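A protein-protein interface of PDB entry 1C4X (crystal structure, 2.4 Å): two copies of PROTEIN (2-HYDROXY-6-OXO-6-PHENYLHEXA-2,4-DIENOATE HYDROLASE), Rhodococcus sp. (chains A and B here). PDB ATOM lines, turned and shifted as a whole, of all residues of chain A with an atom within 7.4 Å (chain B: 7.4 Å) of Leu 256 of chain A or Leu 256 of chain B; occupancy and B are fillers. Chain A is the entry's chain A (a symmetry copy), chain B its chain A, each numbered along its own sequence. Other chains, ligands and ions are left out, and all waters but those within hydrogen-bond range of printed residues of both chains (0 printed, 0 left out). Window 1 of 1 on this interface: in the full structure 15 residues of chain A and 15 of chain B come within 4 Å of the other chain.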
ATOM      1  N   LEU A 133      -5.593  17.811  30.923  1.00  0.00           N
ATOM      2  CA  LEU A 133      -6.070  18.978  30.197  1.00  0.00           C
ATOM      3  C   LEU A 133      -6.769  18.533  28.927  1.00  0.00           C
ATOM      4  O   LEU A 133      -6.385  17.536  28.323  1.00  0.00           O
ATOM      5  CB  LEU A 133      -4.897  19.890  29.819  1.00  0.00           C
ATOM      6  CG  LEU A 133      -3.853  20.226  30.885  1.00  0.00           C
ATOM      7  CD1 LEU A 133      -2.549  20.649  30.240  1.00  0.00           C
ATOM      8  CD2 LEU A 133      -4.375  21.342  31.760  1.00  0.00           C
ATOM      9  N   VAL A 228       1.285  14.859  33.152  1.00  0.00           N
ATOM     10  CA  VAL A 228       0.163  15.450  32.433  1.00  0.00           C
ATOM     11  C   VAL A 228      -0.381  14.546  31.327  1.00  0.00           C
ATOM     12  O   VAL A 228       0.365  13.945  30.564  1.00  0.00           O
ATOM     13  CB  VAL A 228       0.546  16.812  31.802  1.00  0.00           C
ATOM     14  CG1 VAL A 228      -0.716  17.585  31.445  1.00  0.00           C
ATOM     15  CG2 VAL A 228       1.426  17.610  32.759  1.00  0.00           C
ATOM     16  N   LEU A 229      -1.701  14.459  31.266  1.00  0.00           N
ATOM     17  CA  LEU A 229      -2.396  13.672  30.272  1.00  0.00           C
ATOM     18  C   LEU A 229      -3.169  14.712  29.468  1.00  0.00           C
ATOM     19  O   LEU A 229      -4.095  15.346  29.985  1.00  0.00           O
ATOM     20  CB  LEU A 229      -3.355  12.698  30.959  1.00  0.00           C
ATOM     21  CG  LEU A 229      -3.669  11.349  30.303  1.00  0.00           C
ATOM     22  CD1 LEU A 229      -5.053  10.916  30.738  1.00  0.00           C
ATOM     23  CD2 LEU A 229      -3.588  11.441  28.776  1.00  0.00           C
ATOM     24  N   VAL A 230      -2.779  14.893  28.208  1.00  0.00           N
ATOM     25  CA  VAL A 230      -3.405  15.882  27.335  1.00  0.00           C
ATOM     26  C   VAL A 230      -4.447  15.239  26.431  1.00  0.00           C
ATOM     27  O   VAL A 230      -4.178  14.234  25.793  1.00  0.00           O
ATOM     28  CB  VAL A 230      -2.326  16.600  26.461  1.00  0.00           C
ATOM     29  CG1 VAL A 230      -2.926  17.819  25.751  1.00  0.00           C
ATOM     30  CG2 VAL A 230      -1.157  17.018  27.330  1.00  0.00           C
ATOM     31  N   PHE A 231      -5.637  15.818  26.387  1.00  0.00           N
ATOM     32  CA  PHE A 231      -6.712  15.307  25.550  1.00  0.00           C
ATOM     33  C   PHE A 231      -7.094  16.387  24.572  1.00  0.00           C
ATOM     34  O   PHE A 231      -7.050  17.558  24.911  1.00  0.00           O
ATOM     35  CB  PHE A 231      -7.957  14.996  26.374  1.00  0.00           C
ATOM     36  CG  PHE A 231      -7.855  13.766  27.207  1.00  0.00           C
ATOM     37  CD1 PHE A 231      -7.630  13.858  28.575  1.00  0.00           C
ATOM     38  CD2 PHE A 231      -8.020  12.507  26.636  1.00  0.00           C
ATOM     39  CE1 PHE A 231      -7.573  12.710  29.368  1.00  0.00           C
ATOM     40  CE2 PHE A 231      -7.964  11.345  27.422  1.00  0.00           C
ATOM     41  CZ  PHE A 231      -7.738  11.452  28.791  1.00  0.00           C
ATOM     42  N   HIS A 232      -7.473  15.995  23.364  1.00  0.00           N
ATOM     43  CA  HIS A 232      -7.916  16.942  22.347  1.00  0.00           C
ATOM     44  C   HIS A 232      -8.811  16.201  21.372  1.00  0.00           C
ATOM     45  O   HIS A 232      -8.502  15.093  20.938  1.00  0.00           O
ATOM     46  CB  HIS A 232      -6.734  17.583  21.604  1.00  0.00           C
ATOM     47  CG  HIS A 232      -7.005  18.983  21.132  1.00  0.00           C
ATOM     48  ND1 HIS A 232      -6.309  20.078  21.596  1.00  0.00           N
ATOM     49  CD2 HIS A 232      -7.919  19.468  20.254  1.00  0.00           C
ATOM     50  CE1 HIS A 232      -6.780  21.173  21.026  1.00  0.00           C
ATOM     51  NE2 HIS A 232      -7.758  20.831  20.209  1.00  0.00           N
ATOM     52  N   ARG A 234     -10.453  15.329  17.921  1.00  0.00           N
ATOM     53  CA  ARG A 234      -9.981  15.409  16.550  1.00  0.00           C
ATOM     54  C   ARG A 234     -10.761  16.457  15.749  1.00  0.00           C
ATOM     55  O   ARG A 234     -10.235  17.012  14.778  1.00  0.00           O
ATOM     56  CB  ARG A 234     -10.090  14.035  15.877  1.00  0.00           C
ATOM     57  CG  ARG A 234      -9.294  13.901  14.578  1.00  0.00           C
ATOM     58  CD  ARG A 234      -9.046  12.442  14.198  1.00  0.00           C
ATOM     59  NE  ARG A 234     -10.227  11.837  13.586  1.00  0.00           N
ATOM     60  CZ  ARG A 234     -10.329  11.500  12.303  1.00  0.00           C
ATOM     61  NH1 ARG A 234      -9.317  11.701  11.460  1.00  0.00           N
ATOM     62  NH2 ARG A 234     -11.462  10.968  11.863  1.00  0.00           N
ATOM     63  N   LEU A 241      -5.457  21.890  17.447  1.00  0.00           N
ATOM     64  CA  LEU A 241      -4.599  20.867  18.023  1.00  0.00           C
ATOM     65  C   LEU A 241      -3.185  21.392  18.356  1.00  0.00           C
ATOM     66  O   LEU A 241      -2.474  20.807  19.175  1.00  0.00           O
ATOM     67  CB  LEU A 241      -4.522  19.690  17.051  1.00  0.00           C
ATOM     68  CG  LEU A 241      -3.842  18.403  17.512  1.00  0.00           C
ATOM     69  CD1 LEU A 241      -4.661  17.729  18.597  1.00  0.00           C
ATOM     70  CD2 LEU A 241      -3.683  17.491  16.323  1.00  0.00           C
ATOM     71  N   THR A 243      -2.256  23.723  20.172  1.00  0.00           N
ATOM     72  CA  THR A 243      -2.060  24.020  21.589  1.00  0.00           C
ATOM     73  C   THR A 243      -1.594  22.769  22.348  1.00  0.00           C
ATOM     74  O   THR A 243      -0.583  22.812  23.057  1.00  0.00           O
ATOM     75  CB  THR A 243      -3.348  24.611  22.228  1.00  0.00           C
ATOM     76  OG1 THR A 243      -4.400  23.644  22.189  1.00  0.00           O
ATOM     77  CG2 THR A 243      -3.786  25.861  21.471  1.00  0.00           C
ATOM     78  N   SER A 244      -2.306  21.654  22.168  1.00  0.00           N
ATOM     79  CA  SER A 244      -1.957  20.391  22.824  1.00  0.00           C
ATOM     80  C   SER A 244      -0.590  19.873  22.391  1.00  0.00           C
ATOM     81  O   SER A 244       0.160  19.332  23.194  1.00  0.00           O
ATOM     82  CB  SER A 244      -3.015  19.329  22.528  1.00  0.00           C
ATOM     83  OG  SER A 244      -4.287  19.762  22.956  1.00  0.00           O
ATOM     84  N   LEU A 245      -0.265  20.038  21.118  1.00  0.00           N
ATOM     85  CA  LEU A 245       1.018  19.571  20.619  1.00  0.00           C
ATOM     86  C   LEU A 245       2.152  20.338  21.267  1.00  0.00           C
ATOM     87  O   LEU A 245       3.188  19.749  21.594  1.00  0.00           O
ATOM     88  CB  LEU A 245       1.101  19.735  19.099  1.00  0.00           C
ATOM     89  CG  LEU A 245       0.167  18.869  18.250  1.00  0.00           C
ATOM     90  CD1 LEU A 245       0.254  19.313  16.811  1.00  0.00           C
ATOM     91  CD2 LEU A 245       0.536  17.409  18.378  1.00  0.00           C
ATOM     92  N   THR A 248       2.392  19.113  24.772  1.00  0.00           N
ATOM     93  CA  THR A 248       2.925  17.753  24.777  1.00  0.00           C
ATOM     94  C   THR A 248       4.404  17.741  24.419  1.00  0.00           C
ATOM     95  O   THR A 248       5.156  16.886  24.874  1.00  0.00           O
ATOM     96  CB  THR A 248       2.177  16.839  23.791  1.00  0.00           C
ATOM     97  OG1 THR A 248       0.772  16.898  24.060  1.00  0.00           O
ATOM     98  CG2 THR A 248       2.646  15.394  23.947  1.00  0.00           C
ATOM     99  N   ALA A 254       4.412  14.096  29.755  1.00  0.00           N
ATOM    100  CA  ALA A 254       3.127  14.268  29.085  1.00  0.00           C
ATOM    101  C   ALA A 254       2.844  13.171  28.076  1.00  0.00           C
ATOM    102  O   ALA A 254       3.749  12.538  27.548  1.00  0.00           O
ATOM    103  CB  ALA A 254       3.067  15.643  28.389  1.00  0.00           C
ATOM    104  N   GLU A 255       1.562  12.952  27.832  1.00  0.00           N
ATOM    105  CA  GLU A 255       1.115  11.980  26.855  1.00  0.00           C
ATOM    106  C   GLU A 255      -0.127  12.585  26.231  1.00  0.00           C
ATOM    107  O   GLU A 255      -0.945  13.182  26.927  1.00  0.00           O
ATOM    108  CB  GLU A 255       0.820  10.636  27.522  1.00  0.00           C
ATOM    109  CG  GLU A 255       2.106   9.876  27.822  1.00  0.00           C
ATOM    110  CD  GLU A 255       1.887   8.432  28.236  1.00  0.00           C
ATOM    111  OE1 GLU A 255       2.835   7.630  28.092  1.00  0.00           O
ATOM    112  OE2 GLU A 255       0.780   8.100  28.706  1.00  0.00           O
ATOM    113  N   LEU A 256      -0.240  12.465  24.911  1.00  0.00           N
ATOM    114  CA  LEU A 256      -1.374  13.015  24.184  1.00  0.00           C
ATOM    115  C   LEU A 256      -2.294  11.940  23.618  1.00  0.00           C
ATOM    116  O   LEU A 256      -1.837  10.942  23.073  1.00  0.00           O
ATOM    117  CB  LEU A 256      -0.872  13.915  23.051  1.00  0.00           C
ATOM    118  CG  LEU A 256      -1.962  14.452  22.123  1.00  0.00           C
ATOM    119  CD1 LEU A 256      -2.728  15.580  22.794  1.00  0.00           C
ATOM    120  CD2 LEU A 256      -1.326  14.941  20.859  1.00  0.00           C
ATOM    121  N   VAL A 257      -3.596  12.156  23.769  1.00  0.00           N
ATOM    122  CA  VAL A 257      -4.617  11.256  23.264  1.00  0.00           C
ATOM    123  C   VAL A 257      -5.568  12.134  22.445  1.00  0.00           C
ATOM    124  O   VAL A 257      -6.095  13.114  22.966  1.00  0.00           O
ATOM    125  CB  VAL A 257      -5.407  10.590  24.418  1.00  0.00           C
ATOM    126  CG1 VAL A 257      -6.486   9.695  23.861  1.00  0.00           C
ATOM    127  CG2 VAL A 257      -4.486   9.790  25.289  1.00  0.00           C
ATOM    128  N   VAL A 258      -5.769  11.807  21.169  1.00  0.00           N
ATOM    129  CA  VAL A 258      -6.662  12.584  20.302  1.00  0.00           C
ATOM    130  C   VAL A 258      -7.877  11.744  19.974  1.00  0.00           C
ATOM    131  O   VAL A 258      -7.792  10.820  19.185  1.00  0.00           O
ATOM    132  CB  VAL A 258      -5.989  12.950  18.978  1.00  0.00           C
ATOM    133  CG1 VAL A 258      -6.946  13.769  18.130  1.00  0.00           C
ATOM    134  CG2 VAL A 258      -4.699  13.695  19.238  1.00  0.00           C
ATOM    135  N   LEU A 259      -9.014  12.076  20.561  1.00  0.00           N
ATOM    136  CA  LEU A 259     -10.233  11.314  20.354  1.00  0.00           C
ATOM    137  C   LEU A 259     -10.973  11.641  19.071  1.00  0.00           C
ATOM    138  O   LEU A 259     -10.967  12.776  18.605  1.00  0.00           O
ATOM    139  CB  LEU A 259     -11.166  11.526  21.550  1.00  0.00           C
ATOM    140  CG  LEU A 259     -10.514  11.223  22.902  1.00  0.00           C
ATOM    141  CD1 LEU A 259     -11.376  11.724  24.044  1.00  0.00           C
ATOM    142  CD2 LEU A 259     -10.294   9.722  23.006  1.00  0.00           C
ATOM    143  N   ASP A 260     -11.627  10.635  18.510  1.00  0.00           N
ATOM    144  CA  ASP A 260     -12.390  10.817  17.285  1.00  0.00           C
ATOM    145  C   ASP A 260     -13.839  11.115  17.644  1.00  0.00           C
ATOM    146  O   ASP A 260     -14.248  10.869  18.779  1.00  0.00           O
ATOM    147  CB  ASP A 260     -12.320   9.551  16.425  1.00  0.00           C
ATOM    148  CG  ASP A 260     -12.689   9.810  14.980  1.00  0.00           C
ATOM    149  OD1 ASP A 260     -13.149   8.865  14.311  1.00  0.00           O
ATOM    150  OD2 ASP A 260     -12.524  10.960  14.512  1.00  0.00           O
ATOM    151  N   LEU B 133      -1.156   1.416  13.671  1.00  0.00           N
ATOM    152  CA  LEU B 133       0.130   1.812  13.120  1.00  0.00           C
ATOM    153  C   LEU B 133       0.952   2.495  14.195  1.00  0.00           C
ATOM    154  O   LEU B 133       0.406   3.177  15.057  1.00  0.00           O
ATOM    155  CB  LEU B 133      -0.064   2.789  11.954  1.00  0.00           C
ATOM    156  CG  LEU B 133      -1.105   2.459  10.883  1.00  0.00           C
ATOM    157  CD1 LEU B 133      -1.539   3.716  10.157  1.00  0.00           C
ATOM    158  CD2 LEU B 133      -0.513   1.478   9.898  1.00  0.00           C
ATOM    159  N   VAL B 228      -8.682   3.119  12.463  1.00  0.00           N
ATOM    160  CA  VAL B 228      -7.240   3.144  12.678  1.00  0.00           C
ATOM    161  C   VAL B 228      -6.847   3.756  14.022  1.00  0.00           C
ATOM    162  O   VAL B 228      -7.374   4.780  14.440  1.00  0.00           O
ATOM    163  CB  VAL B 228      -6.512   3.927  11.557  1.00  0.00           C
ATOM    164  CG1 VAL B 228      -5.030   3.578  11.567  1.00  0.00           C
ATOM    165  CG2 VAL B 228      -7.140   3.616  10.201  1.00  0.00           C
ATOM    166  N   LEU B 229      -5.913   3.100  14.692  1.00  0.00           N
ATOM    167  CA  LEU B 229      -5.398   3.540  15.969  1.00  0.00           C
ATOM    168  C   LEU B 229      -3.930   3.839  15.678  1.00  0.00           C
ATOM    169  O   LEU B 229      -3.148   2.928  15.388  1.00  0.00           O
ATOM    170  CB  LEU B 229      -5.527   2.415  16.997  1.00  0.00           C
ATOM    171  CG  LEU B 229      -5.734   2.756  18.476  1.00  0.00           C
ATOM    172  CD1 LEU B 229      -5.156   1.633  19.312  1.00  0.00           C
ATOM    173  CD2 LEU B 229      -5.076   4.092  18.837  1.00  0.00           C
ATOM    174  N   VAL B 230      -3.565   5.118  15.746  1.00  0.00           N
ATOM    175  CA  VAL B 230      -2.201   5.552  15.456  1.00  0.00           C
ATOM    176  C   VAL B 230      -1.397   5.736  16.736  1.00  0.00           C
ATOM    177  O   VAL B 230      -1.850   6.386  17.664  1.00  0.00           O
ATOM    178  CB  VAL B 230      -2.215   6.891  14.650  1.00  0.00           C
ATOM    179  CG1 VAL B 230      -0.818   7.210  14.103  1.00  0.00           C
ATOM    180  CG2 VAL B 230      -3.215   6.797  13.515  1.00  0.00           C
ATOM    181  N   PHE B 231      -0.208   5.155  16.780  1.00  0.00           N
ATOM    182  CA  PHE B 231       0.661   5.270  17.941  1.00  0.00           C
ATOM    183  C   PHE B 231       1.943   5.926  17.500  1.00  0.00           C
ATOM    184  O   PHE B 231       2.390   5.702  16.388  1.00  0.00           O
ATOM    185  CB  PHE B 231       1.035   3.897  18.493  1.00  0.00           C
ATOM    186  CG  PHE B 231      -0.062   3.209  19.228  1.00  0.00           C
ATOM    187  CD1 PHE B 231      -0.774   2.177  18.627  1.00  0.00           C
ATOM    188  CD2 PHE B 231      -0.367   3.561  20.540  1.00  0.00           C
ATOM    189  CE1 PHE B 231      -1.776   1.501  19.325  1.00  0.00           C
ATOM    190  CE2 PHE B 231      -1.373   2.888  21.252  1.00  0.00           C
ATOM    191  CZ  PHE B 231      -2.077   1.857  20.638  1.00  0.00           C
ATOM    192  N   HIS B 232       2.536   6.731  18.372  1.00  0.00           N
ATOM    193  CA  HIS B 232       3.807   7.382  18.082  1.00  0.00           C
ATOM    194  C   HIS B 232       4.484   7.702  19.402  1.00  0.00           C
ATOM    195  O   HIS B 232       3.857   8.198  20.336  1.00  0.00           O
ATOM    196  CB  HIS B 232       3.621   8.664  17.254  1.00  0.00           C
ATOM    197  CG  HIS B 232       4.773   8.963  16.338  1.00  0.00           C
ATOM    198  ND1 HIS B 232       4.653   8.980  14.965  1.00  0.00           N
ATOM    199  CD2 HIS B 232       6.077   9.231  16.600  1.00  0.00           C
ATOM    200  CE1 HIS B 232       5.829   9.245  14.424  1.00  0.00           C
ATOM    201  NE2 HIS B 232       6.710   9.401  15.394  1.00  0.00           N
ATOM    202  N   ARG B 234       6.714   9.708  21.926  1.00  0.00           N
ATOM    203  CA  ARG B 234       7.015  11.120  22.078  1.00  0.00           C
ATOM    204  C   ARG B 234       8.489  11.413  21.783  1.00  0.00           C
ATOM    205  O   ARG B 234       8.831  12.532  21.386  1.00  0.00           O
ATOM    206  CB  ARG B 234       6.652  11.584  23.495  1.00  0.00           C
ATOM    207  CG  ARG B 234       6.573  13.102  23.663  1.00  0.00           C
ATOM    208  CD  ARG B 234       5.779  13.508  24.904  1.00  0.00           C
ATOM    209  NE  ARG B 234       6.577  13.372  26.121  1.00  0.00           N
ATOM    210  CZ  ARG B 234       7.032  14.389  26.848  1.00  0.00           C
ATOM    211  NH1 ARG B 234       6.777  15.650  26.497  1.00  0.00           N
ATOM    212  NH2 ARG B 234       7.757  14.137  27.929  1.00  0.00           N
ATOM    213  N   LEU B 241       6.822  12.998  14.351  1.00  0.00           N
ATOM    214  CA  LEU B 241       5.402  12.938  14.660  1.00  0.00           C
ATOM    215  C   LEU B 241       4.516  13.431  13.496  1.00  0.00           C
ATOM    216  O   LEU B 241       3.331  13.101  13.424  1.00  0.00           O
ATOM    217  CB  LEU B 241       5.142  13.760  15.922  1.00  0.00           C
ATOM    218  CG  LEU B 241       3.760  13.692  16.567  1.00  0.00           C
ATOM    219  CD1 LEU B 241       3.517  12.316  17.158  1.00  0.00           C
ATOM    220  CD2 LEU B 241       3.677  14.751  17.637  1.00  0.00           C
ATOM    221  N   THR B 243       4.298  12.472  10.558  1.00  0.00           N
ATOM    222  CA  THR B 243       3.696  11.391   9.782  1.00  0.00           C
ATOM    223  C   THR B 243       2.357  10.958  10.399  1.00  0.00           C
ATOM    224  O   THR B 243       1.339  10.902   9.700  1.00  0.00           O
ATOM    225  CB  THR B 243       4.664  10.181   9.648  1.00  0.00           C
ATOM    226  OG1 THR B 243       4.923   9.619  10.936  1.00  0.00           O
ATOM    227  CG2 THR B 243       5.980  10.628   9.020  1.00  0.00           C
ATOM    228  N   SER B 244       2.354  10.692  11.707  1.00  0.00           N
ATOM    229  CA  SER B 244       1.138  10.283  12.417  1.00  0.00           C
ATOM    230  C   SER B 244       0.063  11.363  12.390  1.00  0.00           C
ATOM    231  O   SER B 244      -1.120  11.069  12.270  1.00  0.00           O
ATOM    232  CB  SER B 244       1.464   9.932  13.867  1.00  0.00           C
ATOM    233  OG  SER B 244       2.428   8.904  13.925  1.00  0.00           O
ATOM    234  N   LEU B 245       0.473  12.617  12.505  1.00  0.00           N
ATOM    235  CA  LEU B 245      -0.486  13.710  12.492  1.00  0.00           C
ATOM    236  C   LEU B 245      -1.179  13.795  11.148  1.00  0.00           C
ATOM    237  O   LEU B 245      -2.385  14.054  11.090  1.00  0.00           O
ATOM    238  CB  LEU B 245       0.207  15.043  12.789  1.00  0.00           C
ATOM    239  CG  LEU B 245       0.790  15.230  14.192  1.00  0.00           C
ATOM    240  CD1 LEU B 245       1.593  16.506  14.226  1.00  0.00           C
ATOM    241  CD2 LEU B 245      -0.315  15.272  15.224  1.00  0.00           C
ATOM    242  N   THR B 248      -3.540  10.924  10.989  1.00  0.00           N
ATOM    243  CA  THR B 248      -4.656  11.161  11.903  1.00  0.00           C
ATOM    244  C   THR B 248      -5.574  12.255  11.377  1.00  0.00           C
ATOM    245  O   THR B 248      -6.774  12.244  11.628  1.00  0.00           O
ATOM    246  CB  THR B 248      -4.173  11.563  13.307  1.00  0.00           C
ATOM    247  OG1 THR B 248      -3.243  10.585  13.788  1.00  0.00           O
ATOM    248  CG2 THR B 248      -5.354  11.635  14.273  1.00  0.00           C
ATOM    249  N   ALA B 254      -9.865   7.635  12.794  1.00  0.00           N
ATOM    250  CA  ALA B 254      -8.551   7.518  13.419  1.00  0.00           C
ATOM    251  C   ALA B 254      -8.492   8.182  14.781  1.00  0.00           C
ATOM    252  O   ALA B 254      -9.254   9.091  15.084  1.00  0.00           O
ATOM    253  CB  ALA B 254      -7.467   8.119  12.500  1.00  0.00           C
ATOM    254  N   GLU B 255      -7.577   7.694  15.603  1.00  0.00           N
ATOM    255  CA  GLU B 255      -7.346   8.247  16.922  1.00  0.00           C
ATOM    256  C   GLU B 255      -5.852   8.130  17.148  1.00  0.00           C
ATOM    257  O   GLU B 255      -5.245   7.124  16.786  1.00  0.00           O
ATOM    258  CB  GLU B 255      -8.144   7.483  17.978  1.00  0.00           C
ATOM    259  CG  GLU B 255      -9.612   7.892  17.964  1.00  0.00           C
ATOM    260  CD  GLU B 255     -10.407   7.378  19.150  1.00  0.00           C
ATOM    261  OE1 GLU B 255     -11.459   7.981  19.458  1.00  0.00           O
ATOM    262  OE2 GLU B 255      -9.990   6.378  19.769  1.00  0.00           O
ATOM    263  N   LEU B 256      -5.257   9.179  17.708  1.00  0.00           N
ATOM    264  CA  LEU B 256      -3.825   9.204  17.965  1.00  0.00           C
ATOM    265  C   LEU B 256      -3.488   9.154  19.451  1.00  0.00           C
ATOM    266  O   LEU B 256      -4.114   9.825  20.262  1.00  0.00           O
ATOM    267  CB  LEU B 256      -3.211  10.459  17.338  1.00  0.00           C
ATOM    268  CG  LEU B 256      -1.730  10.676  17.649  1.00  0.00           C
ATOM    269  CD1 LEU B 256      -0.866   9.737  16.824  1.00  0.00           C
ATOM    270  CD2 LEU B 256      -1.375  12.100  17.351  1.00  0.00           C
ATOM    271  N   VAL B 257      -2.498   8.337  19.791  1.00  0.00           N
ATOM    272  CA  VAL B 257      -2.021   8.187  21.154  1.00  0.00           C
ATOM    273  C   VAL B 257      -0.506   8.398  21.083  1.00  0.00           C
ATOM    274  O   VAL B 257       0.172   7.708  20.324  1.00  0.00           O
ATOM    275  CB  VAL B 257      -2.311   6.768  21.703  1.00  0.00           C
ATOM    276  CG1 VAL B 257      -1.766   6.631  23.104  1.00  0.00           C
ATOM    277  CG2 VAL B 257      -3.786   6.499  21.706  1.00  0.00           C
ATOM    278  N   VAL B 258       0.023   9.356  21.843  1.00  0.00           N
ATOM    279  CA  VAL B 258       1.463   9.636  21.847  1.00  0.00           C
ATOM    280  C   VAL B 258       2.035   9.235  23.189  1.00  0.00           C
ATOM    281  O   VAL B 258       1.824   9.916  24.176  1.00  0.00           O
ATOM    282  CB  VAL B 258       1.752  11.126  21.654  1.00  0.00           C
ATOM    283  CG1 VAL B 258       3.253  11.357  21.644  1.00  0.00           C
ATOM    284  CG2 VAL B 258       1.104  11.621  20.381  1.00  0.00           C
ATOM    285  N   LEU B 259       2.778   8.142  23.223  1.00  0.00           N
ATOM    286  CA  LEU B 259       3.341   7.639  24.464  1.00  0.00           C
ATOM    287  C   LEU B 259       4.612   8.337  24.910  1.00  0.00           C
ATOM    288  O   LEU B 259       5.419   8.771  24.093  1.00  0.00           O
ATOM    289  CB  LEU B 259       3.606   6.137  24.322  1.00  0.00           C
ATOM    290  CG  LEU B 259       2.381   5.335  23.873  1.00  0.00           C
ATOM    291  CD1 LEU B 259       2.773   3.927  23.473  1.00  0.00           C
ATOM    292  CD2 LEU B 259       1.373   5.315  25.012  1.00  0.00           C
ATOM    293  N   ASP B 260       4.792   8.427  26.219  1.00  0.00           N
ATOM    294  CA  ASP B 260       5.976   9.059  26.780  1.00  0.00           C
ATOM    295  C   ASP B 260       7.026   7.990  27.050  1.00  0.00           C
ATOM    296  O   ASP B 260       6.693   6.805  27.085  1.00  0.00           O
ATOM    297  CB  ASP B 260       5.624   9.780  28.084  1.00  0.00           C
ATOM    298  CG  ASP B 260       6.662  10.811  28.476  1.00  0.00           C
ATOM    299  OD1 ASP B 260       6.781  11.098  29.682  1.00  0.00           O
ATOM    300  OD2 ASP B 260       7.363  11.332  27.577  1.00  0.00           O
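The backbone carbonyl oxygen (O) of Val 228 of chain A is in hydrogen-bond range of the backbone NH (N) of Glu 255 of chain A (3.1 Å).
The backbone carbonyl oxygen (O) of Leu 259 of chain A lies within hydrogen-bond range of the backbone NH (N) of Arg 234 of chain A (2.7 Å).
The backbone carbonyl oxygen of His 232 of chain B is in hydrogen-bond range of the backbone NH of Leu 259 of chain B (3.1 Å).
Hydrophobic or aromatic side chains of chain B within 4 Å of the printed part of chain A: Leu 245 and Val 258.
Hydrophobic or aromatic side chains of chain A that line the printed part of chain B: Leu 245 and Val 258.
Among the printed residues, 18 pairs touch across the chains.
Among the printed residues, no Asp or Glu carboxylate lies within 4 Å of a Lys or Arg side-chain nitrogen of the other chain.
Thr 243 of chain A touches none of the printed residues of chain B.
Printed residues of chain B within 4 Å of Leu 245 of chain A: Leu 245.
Printed residues of chain B within 4 Å of Ala 254 of chain A: Arg 234 and Asp 260.
Of chain B, only Leu 256, Val 257 and Val 258 come within 4 Å of Leu 256 of chain A.
Of the printed residues of chain B, Leu 259 of chain A touches Glu 255 (3.7 Å).
Printed residues of chain A within 4 Å of Glu 255 of chain B: Val 258, Leu 259 and Asp 260.
Of chain A, only Leu 256 (3.8 Å), Val 257 (3.4 Å) and Val 258 (2.7 Å) come within 4 Å of Leu 256 of chain B.
The nearest residue of chain B that does not touch Leu 256 of chain A is Leu 259 of chain B (5.4 Å).
The nearest residue of chain A that does not touch Leu 256 of chain B is Leu 259 of chain A (5.4 Å).
The nearest printed residue of chain B that does not touch Val 257 of chain A is Val 257 of chain B (4.5 Å).
Glu 255 of chain A touches Leu 259 of chain B, and with the chains exchanged Leu 259 of chain A touches Glu 255 of chain B.
Leu 256 of chain A touches Val 257 of chain B, and with the chains exchanged Val 257 of chain A touches Leu 256 of chain B.
Of the 18 pairs that touch across the chains among the printed residues, 18 have their exchanged pair printed and touching as well.
Among the printed residues, pairs that only touch across the chains: Leu 256 of chain A with Val 257 of chain B (3.4 Å), Val 257 of chain A with Leu 256 of chain B (3.4 Å), Ala 254 of chain A with Asp 260 of chain B (3.4 Å), Asp 260 of chain A with Ala 254 of chain B (3.4 Å), Glu 255 of chain A with Val 258 of chain B (3.5 Å), Val 258 of chain A with Glu 255 of chain B (3.5 Å), Leu 259 of chain A with Glu 255 of chain B (3.7 Å), Glu 255 of chain A with Leu 259 of chain B (3.7 Å), Leu 256 of chain A with Leu 256 of chain B (3.8 Å) and Leu 245 of chain A with Leu 245 of chain B (3.9 Å).
O of Ala 254 of chain B is in hydrogen-bond range of NE of Arg 234 of chain A (3.3 Å).
N of Asp 260 of chain A is in hydrogen-bond range of OE1 of Glu 255 of chain B (2.8 Å).
NE of Arg 234 of chain B is in hydrogen-bond range of O of Ala 254 of chain A, at 3.3 Å.
The backbone NH (N) of Val 258 of chain B is in hydrogen-bond range of the backbone carbonyl oxygen (O) of Leu 256 of chain A, 2.7 Å away.
The backbone carbonyl oxygen (O) of Thr 248 of chain B is in hydrogen-bond range of the guanidinium group (NH1) of Arg 234 of chain A (2.6 Å).
The guanidinium group (NH1) of Arg 234 of chain B is in hydrogen-bond range of the backbone carbonyl oxygen (O) of Thr 248 of chain A, at 2.6 Å.
The backbone NH (N) of Asp 260 of chain B sits at hydrogen-bond distance from the side-chain carboxylate (OE1) of Glu 255 of chain A.
The backbone carbonyl oxygen (O) of Leu 256 of chain B is in hydrogen-bond range of the backbone NH (N) of Val 258 of chain A, 2.7 Å away.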
